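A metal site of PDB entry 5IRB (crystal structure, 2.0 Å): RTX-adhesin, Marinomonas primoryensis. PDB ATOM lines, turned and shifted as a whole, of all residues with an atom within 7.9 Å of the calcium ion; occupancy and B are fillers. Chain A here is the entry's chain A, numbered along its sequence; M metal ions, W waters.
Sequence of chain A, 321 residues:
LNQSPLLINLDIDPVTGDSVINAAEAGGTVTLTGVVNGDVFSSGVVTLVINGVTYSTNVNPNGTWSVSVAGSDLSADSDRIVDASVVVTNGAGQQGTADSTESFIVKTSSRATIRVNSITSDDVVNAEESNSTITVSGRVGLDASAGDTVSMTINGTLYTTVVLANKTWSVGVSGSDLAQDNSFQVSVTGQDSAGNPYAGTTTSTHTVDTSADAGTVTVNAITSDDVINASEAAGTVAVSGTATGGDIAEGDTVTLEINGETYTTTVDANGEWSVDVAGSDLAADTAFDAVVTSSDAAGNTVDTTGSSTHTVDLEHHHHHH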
ATOM      1  N   ILE A 222      23.720 -33.510   8.762  1.00  0.00           N
ATOM      2  CA  ILE A 222      23.398 -32.198   9.326  1.00  0.00           C
ATOM      3  C   ILE A 222      23.927 -31.143   8.377  1.00  0.00           C
ATOM      4  O   ILE A 222      25.114 -30.852   8.364  1.00  0.00           O
ATOM      5  CB  ILE A 222      23.991 -32.026  10.727  1.00  0.00           C
ATOM      6  CG1 ILE A 222      23.645 -33.249  11.607  1.00  0.00           C
ATOM      7  CG2 ILE A 222      23.562 -30.699  11.352  1.00  0.00           C
ATOM      8  CD1 ILE A 222      22.186 -33.584  11.659  1.00  0.00           C
ATOM      9  N   THR A 223      23.013 -30.573   7.585  1.00  0.00           N
ATOM     10  CA  THR A 223      23.318 -29.912   6.308  1.00  0.00           C
ATOM     11  C   THR A 223      23.994 -30.911   5.350  1.00  0.00           C
ATOM     12  O   THR A 223      24.309 -32.040   5.727  1.00  0.00           O
ATOM     13  CB  THR A 223      24.205 -28.650   6.479  1.00  0.00           C
ATOM     14  OG1 THR A 223      25.497 -29.029   6.984  1.00  0.00           O
ATOM     15  CG2 THR A 223      23.552 -27.662   7.441  1.00  0.00           C
ATOM     16  N   SER A 224      24.203 -30.493   4.095  1.00  0.00           N
ATOM     17  CA  SER A 224      24.573 -31.441   3.043  1.00  0.00           C
ATOM     18  C   SER A 224      25.935 -32.141   3.266  1.00  0.00           C
ATOM     19  O   SER A 224      26.126 -33.297   2.860  1.00  0.00           O
ATOM     20  CB  SER A 224      24.577 -30.729   1.681  1.00  0.00           C
ATOM     21  OG  SER A 224      25.040 -29.410   1.837  1.00  0.00           O
ATOM     22  N   ASP A 225      26.874 -31.449   3.896  1.00  0.00           N
ATOM     23  CA  ASP A 225      28.184 -32.044   4.167  1.00  0.00           C
ATOM     24  C   ASP A 225      28.360 -32.531   5.607  1.00  0.00           C
ATOM     25  O   ASP A 225      29.453 -32.968   5.972  1.00  0.00           O
ATOM     26  CB  ASP A 225      29.289 -31.046   3.805  1.00  0.00           C
ATOM     27  CG  ASP A 225      29.336 -29.836   4.738  1.00  0.00           C
ATOM     28  OD1 ASP A 225      28.574 -29.756   5.721  1.00  0.00           O
ATOM     29  OD2 ASP A 225      30.145 -28.946   4.466  1.00  0.00           O
ATOM     30  N   ASP A 226      27.305 -32.445   6.412  1.00  0.00           N
ATOM     31  CA  ASP A 226      27.300 -32.985   7.779  1.00  0.00           C
ATOM     32  C   ASP A 226      28.260 -32.183   8.666  1.00  0.00           C
ATOM     33  O   ASP A 226      28.758 -32.686   9.678  1.00  0.00           O
ATOM     34  CB  ASP A 226      27.661 -34.476   7.771  1.00  0.00           C
ATOM     35  CG  ASP A 226      27.144 -35.208   8.990  1.00  0.00           C
ATOM     36  OD1 ASP A 226      26.036 -34.900   9.499  1.00  0.00           O
ATOM     37  OD2 ASP A 226      27.875 -36.126   9.442  1.00  0.00           O
ATOM     38  N   VAL A 227      28.477 -30.921   8.298  1.00  0.00           N
ATOM     39  CA  VAL A 227      29.336 -29.994   9.031  1.00  0.00           C
ATOM     40  C   VAL A 227      28.645 -28.635   9.212  1.00  0.00           C
ATOM     41  O   VAL A 227      28.150 -28.054   8.252  1.00  0.00           O
ATOM     42  CB  VAL A 227      30.690 -29.762   8.298  1.00  0.00           C
ATOM     43  CG1 VAL A 227      31.585 -28.806   9.089  1.00  0.00           C
ATOM     44  CG2 VAL A 227      31.399 -31.091   8.009  1.00  0.00           C
ATOM     45  N   ILE A 228      28.638 -28.102  10.435  1.00  0.00           N
ATOM     46  CA  ILE A 228      28.052 -26.793  10.690  1.00  0.00           C
ATOM     47  C   ILE A 228      29.103 -25.689  10.506  1.00  0.00           C
ATOM     48  O   ILE A 228      30.079 -25.654  11.246  1.00  0.00           O
ATOM     49  CB  ILE A 228      27.469 -26.689  12.121  1.00  0.00           C
ATOM     50  CG1 ILE A 228      26.273 -27.655  12.286  1.00  0.00           C
ATOM     51  CG2 ILE A 228      27.102 -25.259  12.456  1.00  0.00           C
ATOM     52  CD1 ILE A 228      25.036 -27.238  11.525  1.00  0.00           C
ATOM     53  N   ASN A 229      28.912 -24.805   9.532  1.00  0.00           N
ATOM     54  CA  ASN A 229      29.837 -23.680   9.351  1.00  0.00           C
ATOM     55  C   ASN A 229      29.409 -22.485  10.202  1.00  0.00           C
ATOM     56  O   ASN A 229      28.343 -22.520  10.834  1.00  0.00           O
ATOM     57  CB  ASN A 229      29.956 -23.297   7.865  1.00  0.00           C
ATOM     58  CG  ASN A 229      28.625 -22.851   7.234  1.00  0.00           C
ATOM     59  OD1 ASN A 229      27.804 -22.214   7.882  1.00  0.00           O
ATOM     60  ND2 ASN A 229      28.422 -23.201   5.967  1.00  0.00           N
ATOM     61  N   GLU A 232      25.917 -21.287   8.819  1.00  0.00           N
ATOM     62  CA  GLU A 232      24.836 -22.191   9.190  1.00  0.00           C
ATOM     63  C   GLU A 232      24.497 -22.088  10.676  1.00  0.00           C
ATOM     64  O   GLU A 232      23.318 -22.100  11.056  1.00  0.00           O
ATOM     65  CB  GLU A 232      25.194 -23.647   8.830  1.00  0.00           C
ATOM     66  CG  GLU A 232      25.080 -23.987   7.342  1.00  0.00           C
ATOM     67  CD  GLU A 232      25.878 -25.222   6.937  1.00  0.00           C
ATOM     68  OE1 GLU A 232      26.711 -25.678   7.733  1.00  0.00           O
ATOM     69  OE2 GLU A 232      25.680 -25.718   5.811  1.00  0.00           O
ATOM     70  N   VAL A 237      18.659 -24.478  10.971  1.00  0.00           N
ATOM     71  CA  VAL A 237      18.981 -25.658  10.180  1.00  0.00           C
ATOM     72  C   VAL A 237      17.853 -26.682  10.230  1.00  0.00           C
ATOM     73  O   VAL A 237      17.363 -27.029  11.314  1.00  0.00           O
ATOM     74  CB  VAL A 237      20.293 -26.311  10.644  1.00  0.00           C
ATOM     75  CG1 VAL A 237      20.455 -27.677  10.022  1.00  0.00           C
ATOM     76  CG2 VAL A 237      21.471 -25.433  10.282  1.00  0.00           C
ATOM     77  N   THR A 311      30.013 -32.626  12.812  1.00  0.00           N
ATOM     78  CA  THR A 311      31.126 -31.770  13.196  1.00  0.00           C
ATOM     79  C   THR A 311      30.833 -30.288  12.918  1.00  0.00           C
ATOM     80  O   THR A 311      29.844 -29.954  12.246  1.00  0.00           O
ATOM     81  CB  THR A 311      32.424 -32.220  12.483  1.00  0.00           C
ATOM     82  OG1 THR A 311      32.207 -32.209  11.068  1.00  0.00           O
ATOM     83  CG2 THR A 311      32.776 -33.653  12.893  1.00  0.00           C
HETATM   84 CA    CA M   1      27.348 -27.669   6.108  1.00  0.00          CA
HETATM   85  O   HOH W   1      26.312 -27.653   3.853  1.00  0.00           O
HETATM   86  O   HOH W   2      29.297 -26.513   5.486  1.00  0.00           O
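The calcium ion is bound by O of Val 227 (2.3 Å), water W2 (2.3 Å), OD1 of Asp 225 (2.5 Å), OG1 of Thr 223 (2.5 Å), water W1 (2.5 Å), OE2 of Glu 232 (2.6 Å) and OE1 of Glu 232 (2.6 Å).
The backbone NH (N) of Asn 229 sits close to the side-chain carboxylate (OE1) of Glu 232.
The backbone NH of Val 227 is in hydrogen-bond range of the backbone carbonyl oxygen of Ile 222 (3.4 Å).
Water W2 lies within hydrogen-bond range of OD2 of Asp 225 (2.8 Å) and ND2 of Asn 229 (3.5 Å).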
